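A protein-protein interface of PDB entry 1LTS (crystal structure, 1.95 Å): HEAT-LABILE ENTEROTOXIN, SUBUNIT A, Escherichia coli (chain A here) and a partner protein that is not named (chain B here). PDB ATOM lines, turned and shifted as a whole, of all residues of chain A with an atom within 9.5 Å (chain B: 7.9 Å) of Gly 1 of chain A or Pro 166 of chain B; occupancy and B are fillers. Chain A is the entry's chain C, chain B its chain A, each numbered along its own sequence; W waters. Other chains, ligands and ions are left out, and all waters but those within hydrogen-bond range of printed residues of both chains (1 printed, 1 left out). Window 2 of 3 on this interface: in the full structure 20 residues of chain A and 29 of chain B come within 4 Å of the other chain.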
ATOM      1  N   GLY A   1       4.160  -0.720  23.131  1.00  0.00           N
ATOM      2  CA  GLY A   1       5.505  -0.157  23.144  1.00  0.00           C
ATOM      3  C   GLY A   1       6.185  -0.673  24.408  1.00  0.00           C
ATOM      4  O   GLY A   1       6.147  -1.889  24.606  1.00  0.00           O
ATOM      5  N   ASP A   2       6.696   0.176  25.315  1.00  0.00           N
ATOM      6  CA  ASP A   2       7.246  -0.280  26.589  1.00  0.00           C
ATOM      7  C   ASP A   2       6.110  -1.002  27.298  1.00  0.00           C
ATOM      8  O   ASP A   2       6.344  -2.063  27.844  1.00  0.00           O
ATOM      9  CB  ASP A   2       7.779   0.968  27.325  1.00  0.00           C
ATOM     10  CG  ASP A   2       7.151   1.445  28.635  1.00  0.00           C
ATOM     11  OD1 ASP A   2       5.989   1.870  28.644  1.00  0.00           O
ATOM     12  OD2 ASP A   2       7.859   1.418  29.649  1.00  0.00           O
ATOM     13  N   THR A   3       4.861  -0.541  27.155  1.00  0.00           N
ATOM     14  CA  THR A   3       3.684  -1.214  27.698  1.00  0.00           C
ATOM     15  C   THR A   3       3.563  -2.666  27.266  1.00  0.00           C
ATOM     16  O   THR A   3       3.157  -3.487  28.063  1.00  0.00           O
ATOM     17  CB  THR A   3       2.407  -0.480  27.265  1.00  0.00           C
ATOM     18  OG1 THR A   3       2.781   0.873  27.452  1.00  0.00           O
ATOM     19  CG2 THR A   3       1.120  -0.804  28.013  1.00  0.00           C
ATOM     20  N   CYS A   4       4.019  -3.039  26.078  1.00  0.00           N
ATOM     21  CA  CYS A   4       3.853  -4.386  25.594  1.00  0.00           C
ATOM     22  C   CYS A   4       4.811  -5.258  26.353  1.00  0.00           C
ATOM     23  O   CYS A   4       4.438  -6.333  26.812  1.00  0.00           O
ATOM     24  CB  CYS A   4       4.179  -4.431  24.153  1.00  0.00           C
ATOM     25  SG  CYS A   4       4.162  -6.050  23.377  1.00  0.00           S
ATOM     26  N   ASN A   5       6.043  -4.823  26.571  1.00  0.00           N
ATOM     27  CA  ASN A   5       6.978  -5.662  27.300  1.00  0.00           C
ATOM     28  C   ASN A   5       6.746  -5.632  28.793  1.00  0.00           C
ATOM     29  O   ASN A   5       7.006  -6.654  29.432  1.00  0.00           O
ATOM     30  CB  ASN A   5       8.418  -5.266  27.050  1.00  0.00           C
ATOM     31  CG  ASN A   5       8.800  -5.555  25.606  1.00  0.00           C
ATOM     32  OD1 ASN A   5       9.154  -4.625  24.872  1.00  0.00           O
ATOM     33  ND2 ASN A   5       8.684  -6.766  25.055  1.00  0.00           N
ATOM     34  N   GLU A   6       6.254  -4.530  29.384  1.00  0.00           N
ATOM     35  CA  GLU A   6       5.945  -4.481  30.802  1.00  0.00           C
ATOM     36  C   GLU A   6       4.741  -5.342  31.060  1.00  0.00           C
ATOM     37  O   GLU A   6       4.792  -6.214  31.926  1.00  0.00           O
ATOM     38  CB  GLU A   6       5.633  -3.096  31.254  1.00  0.00           C
ATOM     39  CG  GLU A   6       6.939  -2.357  31.319  1.00  0.00           C
ATOM     40  CD  GLU A   6       6.802  -0.966  31.916  1.00  0.00           C
ATOM     41  OE1 GLU A   6       6.037  -0.166  31.362  1.00  0.00           O
ATOM     42  OE2 GLU A   6       7.465  -0.690  32.927  1.00  0.00           O
ATOM     43  N   GLU A   7       3.697  -5.168  30.256  1.00  0.00           N
ATOM     44  CA  GLU A   7       2.511  -5.983  30.325  1.00  0.00           C
ATOM     45  C   GLU A   7       2.869  -7.459  30.244  1.00  0.00           C
ATOM     46  O   GLU A   7       2.349  -8.239  31.035  1.00  0.00           O
ATOM     47  CB  GLU A   7       1.591  -5.659  29.189  1.00  0.00           C
ATOM     48  CG  GLU A   7       0.159  -6.029  29.431  1.00  0.00           C
ATOM     49  CD  GLU A   7      -0.626  -5.138  30.394  1.00  0.00           C
ATOM     50  OE1 GLU A   7      -0.099  -4.172  30.961  1.00  0.00           O
ATOM     51  OE2 GLU A   7      -1.810  -5.425  30.554  1.00  0.00           O
ATOM     52  N   THR A   8       3.753  -7.863  29.323  1.00  0.00           N
ATOM     53  CA  THR A   8       4.179  -9.243  29.196  1.00  0.00           C
ATOM     54  C   THR A   8       4.850  -9.699  30.488  1.00  0.00           C
ATOM     55  O   THR A   8       4.539 -10.776  31.008  1.00  0.00           O
ATOM     56  CB  THR A   8       5.144  -9.396  27.968  1.00  0.00           C
ATOM     57  OG1 THR A   8       4.312  -9.264  26.805  1.00  0.00           O
ATOM     58  CG2 THR A   8       5.921 -10.724  27.945  1.00  0.00           C
ATOM     59  N   GLY B 163       5.319 -12.869  24.254  1.00  0.00           N
ATOM     60  CA  GLY B 163       6.450 -11.988  24.455  1.00  0.00           C
ATOM     61  C   GLY B 163       7.088 -11.416  23.202  1.00  0.00           C
ATOM     62  O   GLY B 163       8.168 -10.830  23.268  1.00  0.00           O
ATOM     63  N   PHE B 164       6.447 -11.575  22.051  1.00  0.00           N
ATOM     64  CA  PHE B 164       6.918 -11.003  20.786  1.00  0.00           C
ATOM     65  C   PHE B 164       7.052  -9.501  20.964  1.00  0.00           C
ATOM     66  O   PHE B 164       6.220  -8.922  21.681  1.00  0.00           O
ATOM     67  CB  PHE B 164       5.930 -11.203  19.659  1.00  0.00           C
ATOM     68  CG  PHE B 164       5.550 -12.613  19.269  1.00  0.00           C
ATOM     69  CD1 PHE B 164       6.476 -13.430  18.662  1.00  0.00           C
ATOM     70  CD2 PHE B 164       4.247 -13.039  19.484  1.00  0.00           C
ATOM     71  CE1 PHE B 164       6.087 -14.686  18.262  1.00  0.00           C
ATOM     72  CE2 PHE B 164       3.880 -14.294  19.075  1.00  0.00           C
ATOM     73  CZ  PHE B 164       4.796 -15.117  18.465  1.00  0.00           C
ATOM     74  N   PRO B 165       8.021  -8.783  20.389  1.00  0.00           N
ATOM     75  CA  PRO B 165       8.128  -7.338  20.577  1.00  0.00           C
ATOM     76  C   PRO B 165       6.883  -6.654  20.036  1.00  0.00           C
ATOM     77  O   PRO B 165       6.176  -7.265  19.230  1.00  0.00           O
ATOM     78  CB  PRO B 165       9.436  -7.019  19.875  1.00  0.00           C
ATOM     79  CG  PRO B 165       9.657  -8.137  18.886  1.00  0.00           C
ATOM     80  CD  PRO B 165       9.171  -9.327  19.673  1.00  0.00           C
ATOM     81  N   PRO B 166       6.525  -5.425  20.419  1.00  0.00           N
ATOM     82  CA  PRO B 166       5.220  -4.823  20.110  1.00  0.00           C
ATOM     83  C   PRO B 166       4.915  -4.656  18.631  1.00  0.00           C
ATOM     84  O   PRO B 166       3.779  -4.567  18.190  1.00  0.00           O
ATOM     85  CB  PRO B 166       5.266  -3.517  20.828  1.00  0.00           C
ATOM     86  CG  PRO B 166       6.756  -3.196  20.945  1.00  0.00           C
ATOM     87  CD  PRO B 166       7.361  -4.545  21.236  1.00  0.00           C
ATOM     88  N   ASP B 167       6.001  -4.591  17.876  1.00  0.00           N
ATOM     89  CA  ASP B 167       5.979  -4.389  16.447  1.00  0.00           C
ATOM     90  C   ASP B 167       6.014  -5.688  15.672  1.00  0.00           C
ATOM     91  O   ASP B 167       6.096  -5.642  14.453  1.00  0.00           O
ATOM     92  CB  ASP B 167       7.188  -3.524  16.037  1.00  0.00           C
ATOM     93  CG  ASP B 167       8.596  -4.035  16.410  1.00  0.00           C
ATOM     94  OD1 ASP B 167       8.904  -4.205  17.592  1.00  0.00           O
ATOM     95  OD2 ASP B 167       9.402  -4.237  15.507  1.00  0.00           O
ATOM     96  N   HIS B 168       5.985  -6.860  16.294  1.00  0.00           N
ATOM     97  CA  HIS B 168       6.153  -8.100  15.569  1.00  0.00           C
ATOM     98  C   HIS B 168       4.902  -8.362  14.768  1.00  0.00           C
ATOM     99  O   HIS B 168       3.809  -8.166  15.274  1.00  0.00           O
ATOM    100  CB  HIS B 168       6.378  -9.218  16.556  1.00  0.00           C
ATOM    101  CG  HIS B 168       6.889 -10.486  15.899  1.00  0.00           C
ATOM    102  ND1 HIS B 168       6.223 -11.340  15.111  1.00  0.00           N
ATOM    103  CD2 HIS B 168       8.180 -10.957  16.027  1.00  0.00           C
ATOM    104  CE1 HIS B 168       7.051 -12.307  14.749  1.00  0.00           C
ATOM    105  NE2 HIS B 168       8.219 -12.064  15.307  1.00  0.00           N
ATOM    106  N   GLN B 169       5.019  -8.877  13.552  1.00  0.00           N
ATOM    107  CA  GLN B 169       3.859  -9.194  12.751  1.00  0.00           C
ATOM    108  C   GLN B 169       2.890 -10.138  13.455  1.00  0.00           C
ATOM    109  O   GLN B 169       1.675 -10.070  13.263  1.00  0.00           O
ATOM    110  CB  GLN B 169       4.350  -9.798  11.451  1.00  0.00           C
ATOM    111  CG  GLN B 169       3.310 -10.031  10.339  1.00  0.00           C
ATOM    112  CD  GLN B 169       3.849  -9.993   8.892  1.00  0.00           C
ATOM    113  OE1 GLN B 169       3.425 -10.705   7.964  1.00  0.00           O
ATOM    114  NE2 GLN B 169       4.746  -9.061   8.570  1.00  0.00           N
ATOM    115  N   ALA B 170       3.400 -11.080  14.246  1.00  0.00           N
ATOM    116  CA  ALA B 170       2.523 -11.972  15.013  1.00  0.00           C
ATOM    117  C   ALA B 170       1.361 -11.340  15.785  1.00  0.00           C
ATOM    118  O   ALA B 170       0.238 -11.804  15.654  1.00  0.00           O
ATOM    119  CB  ALA B 170       3.351 -12.750  15.977  1.00  0.00           C
ATOM    120  N   TRP B 171       1.553 -10.239  16.501  1.00  0.00           N
ATOM    121  CA  TRP B 171       0.494  -9.543  17.200  1.00  0.00           C
ATOM    122  C   TRP B 171      -0.669  -9.047  16.337  1.00  0.00           C
ATOM    123  O   TRP B 171      -1.721  -8.617  16.813  1.00  0.00           O
ATOM    124  CB  TRP B 171       1.093  -8.351  17.925  1.00  0.00           C
ATOM    125  CG  TRP B 171       1.902  -8.718  19.158  1.00  0.00           C
ATOM    126  CD1 TRP B 171       3.080  -8.070  19.410  1.00  0.00           C
ATOM    127  CD2 TRP B 171       1.564  -9.648  20.142  1.00  0.00           C
ATOM    128  NE1 TRP B 171       3.495  -8.567  20.553  1.00  0.00           N
ATOM    129  CE2 TRP B 171       2.637  -9.502  21.026  1.00  0.00           C
ATOM    130  CE3 TRP B 171       0.547 -10.574  20.422  1.00  0.00           C
ATOM    131  CZ2 TRP B 171       2.703 -10.269  22.183  1.00  0.00           C
ATOM    132  CZ3 TRP B 171       0.617 -11.339  21.574  1.00  0.00           C
ATOM    133  CH2 TRP B 171       1.690 -11.181  22.440  1.00  0.00           C
ATOM    134  N   ARG B 172      -0.485  -9.026  15.025  1.00  0.00           N
ATOM    135  CA  ARG B 172      -1.497  -8.523  14.130  1.00  0.00           C
ATOM    136  C   ARG B 172      -2.080  -9.706  13.405  1.00  0.00           C
ATOM    137  O   ARG B 172      -2.990  -9.525  12.594  1.00  0.00           O
ATOM    138  CB  ARG B 172      -0.879  -7.518  13.146  1.00  0.00           C
ATOM    139  CG  ARG B 172      -0.207  -6.306  13.804  1.00  0.00           C
ATOM    140  CD  ARG B 172       1.249  -6.618  14.242  1.00  0.00           C
ATOM    141  NE  ARG B 172       1.820  -5.644  15.171  1.00  0.00           N
ATOM    142  CZ  ARG B 172       2.488  -4.550  14.765  1.00  0.00           C
ATOM    143  NH1 ARG B 172       2.708  -4.282  13.467  1.00  0.00           N
ATOM    144  NH2 ARG B 172       2.827  -3.634  15.675  1.00  0.00           N
ATOM    145  N   PRO B 181      -1.550  -8.315  24.472  1.00  0.00           N
ATOM    146  CA  PRO B 181      -1.474  -7.439  25.631  1.00  0.00           C
ATOM    147  C   PRO B 181      -1.630  -5.945  25.298  1.00  0.00           C
ATOM    148  O   PRO B 181      -1.616  -5.505  24.141  1.00  0.00           O
ATOM    149  CB  PRO B 181      -0.120  -7.797  26.252  1.00  0.00           C
ATOM    150  CG  PRO B 181       0.192  -9.202  25.779  1.00  0.00           C
ATOM    151  CD  PRO B 181      -0.380  -9.203  24.385  1.00  0.00           C
ATOM    152  N   GLN B 182      -1.736  -5.111  26.332  1.00  0.00           N
ATOM    153  CA  GLN B 182      -1.791  -3.683  26.125  1.00  0.00           C
ATOM    154  C   GLN B 182      -0.442  -3.222  25.609  1.00  0.00           C
ATOM    155  O   GLN B 182       0.622  -3.403  26.210  1.00  0.00           O
ATOM    156  CB  GLN B 182      -2.098  -2.911  27.420  1.00  0.00           C
ATOM    157  CG  GLN B 182      -3.589  -2.877  27.798  1.00  0.00           C
ATOM    158  CD  GLN B 182      -4.477  -2.012  26.905  1.00  0.00           C
ATOM    159  OE1 GLN B 182      -5.307  -2.499  26.137  1.00  0.00           O
ATOM    160  NE2 GLN B 182      -4.339  -0.696  26.975  1.00  0.00           N
ATOM    161  N   GLY B 183      -0.545  -2.680  24.405  1.00  0.00           N
ATOM    162  CA  GLY B 183       0.587  -2.027  23.787  1.00  0.00           C
ATOM    163  C   GLY B 183       1.376  -2.872  22.813  1.00  0.00           C
ATOM    164  O   GLY B 183       2.507  -2.462  22.469  1.00  0.00           O
ATOM    165  N   CYS B 184       0.815  -4.011  22.413  1.00  0.00           N
ATOM    166  CA  CYS B 184       1.416  -4.913  21.443  1.00  0.00           C
ATOM    167  C   CYS B 184       0.518  -4.895  20.216  1.00  0.00           C
ATOM    168  O   CYS B 184      -0.705  -5.014  20.380  1.00  0.00           O
ATOM    169  CB  CYS B 184       1.448  -6.338  21.963  1.00  0.00           C
ATOM    170  SG  CYS B 184       2.213  -6.525  23.573  1.00  0.00           S
ATOM    171  N   GLY B 185       1.064  -4.724  19.012  1.00  0.00           N
ATOM    172  CA  GLY B 185       0.252  -4.808  17.815  1.00  0.00           C
ATOM    173  C   GLY B 185      -0.796  -3.709  17.714  1.00  0.00           C
ATOM    174  O   GLY B 185      -0.490  -2.527  17.531  1.00  0.00           O
HETATM  175  O   HOH W   1       3.211 -11.417  25.492  1.00  0.00           O
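O of Phe 164 of chain B is in hydrogen-bond range of NE1 of Trp 171 of chain B (3.0 Å). NE1 of Trp 171 of chain B lies close to O of Pro 165 of chain B (3.3 Å). The backbone carbonyl oxygen (O) of Pro 166 of chain B is in hydrogen-bond range of the guanidinium group (NH2) of Arg 172 of chain B (2.8 Å). O of Pro 166 of chain B sits at hydrogen-bond distance from N of Gly 185 of chain B, 2.8 Å away. The backbone carbonyl oxygen (O) of Cys 4 of chain A is in hydrogen-bond range of the side-chain hydroxyl (OG1) of Thr 8 of chain A.
The backbone NH of Cys 4 of chain A sits at hydrogen-bond distance from the backbone carbonyl oxygen of Gln 182 of chain B (3.4 Å). The backbone carbonyl oxygen of Gly 183 of chain B lies within hydrogen-bond range of the backbone NH of Gly 1 of chain A, 2.5 Å away. SG of Cys 4 of chain A forms a disulfide with SG of Cys 184 of chain B, 2.0 Å away. O of Thr 3 of chain A sits close to O of Gln 182 of chain B (3.1 Å).
Pro 166 of chain B touches Gly 1 of chain A. SG of Cys 4 of chain A touches O of Phe 164 of chain B (3.9 Å). Cys 4 of chain A touches Pro 166 of chain B. NE1 of Trp 171 of chain B touches SG of Cys 4 of chain A, 3.8 Å away. Gly 183 of chain B touches Cys 4 of chain A (O to CB, 3.1 Å). Pro 181 of chain B touches Glu 7 of chain A. N of Gln 182 of chain B touches CG of Glu 7 of chain A, 3.7 Å away. Gly 163 of chain B touches Thr 8 of chain A (CA to CG2, 3.7 Å).
Water W1 lies within hydrogen-bond range of the side-chain hydroxyl (OG1) of Thr 8 of chain A (2.8 Å) and the backbone NH (N) of Gly 163 of chain B (2.8 Å).
Of chain B, only Pro 166 (3.8 Å) and Gly 183 (2.5 Å) come within 4 Å of Gly 1 of chain A. No residue of chain A comes within 4 Å of Pro 165 of chain B. Of chain A, only Cys 4 (2.0 Å) comes within 4 Å of Cys 184 of chain B. No residue of chain A comes within 4 Å of Gly 185 of chain B. Of the printed residues of chain B, Thr 8 of chain A touches Gly 163. Of the printed residues of chain B, Thr 3 of chain A touches Gln 182. Printed residues of chain B within 4 Å of Glu 7 of chain A: Pro 181 and Gln 182. Of the printed residues of chain A, Phe 164 of chain B touches Cys 4 (3.9 Å). Of the printed residues of chain B, Cys 4 of chain A touches Phe 164 (3.9 Å), Pro 166 (3.6 Å), Trp 171 (3.8 Å), Gln 182 (3.4 Å), Gly 183 (3.1 Å) and Cys 184 (2.0 Å). Arg 172 of chain B touches none of the printed residues of chain A. His 168 of chain B touches none of the printed residues of chain A. The nearest printed residue of chain A that does not touch Trp 171 of chain B is Thr 8 of chain A (5.0 Å).
Along chain B the printed residues that touch a printed residue of chain A span positions 163 to 184. Among the printed residues, no Asp or Glu carboxylate lies within 4 Å of a Lys or Arg side-chain nitrogen of the other chain.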
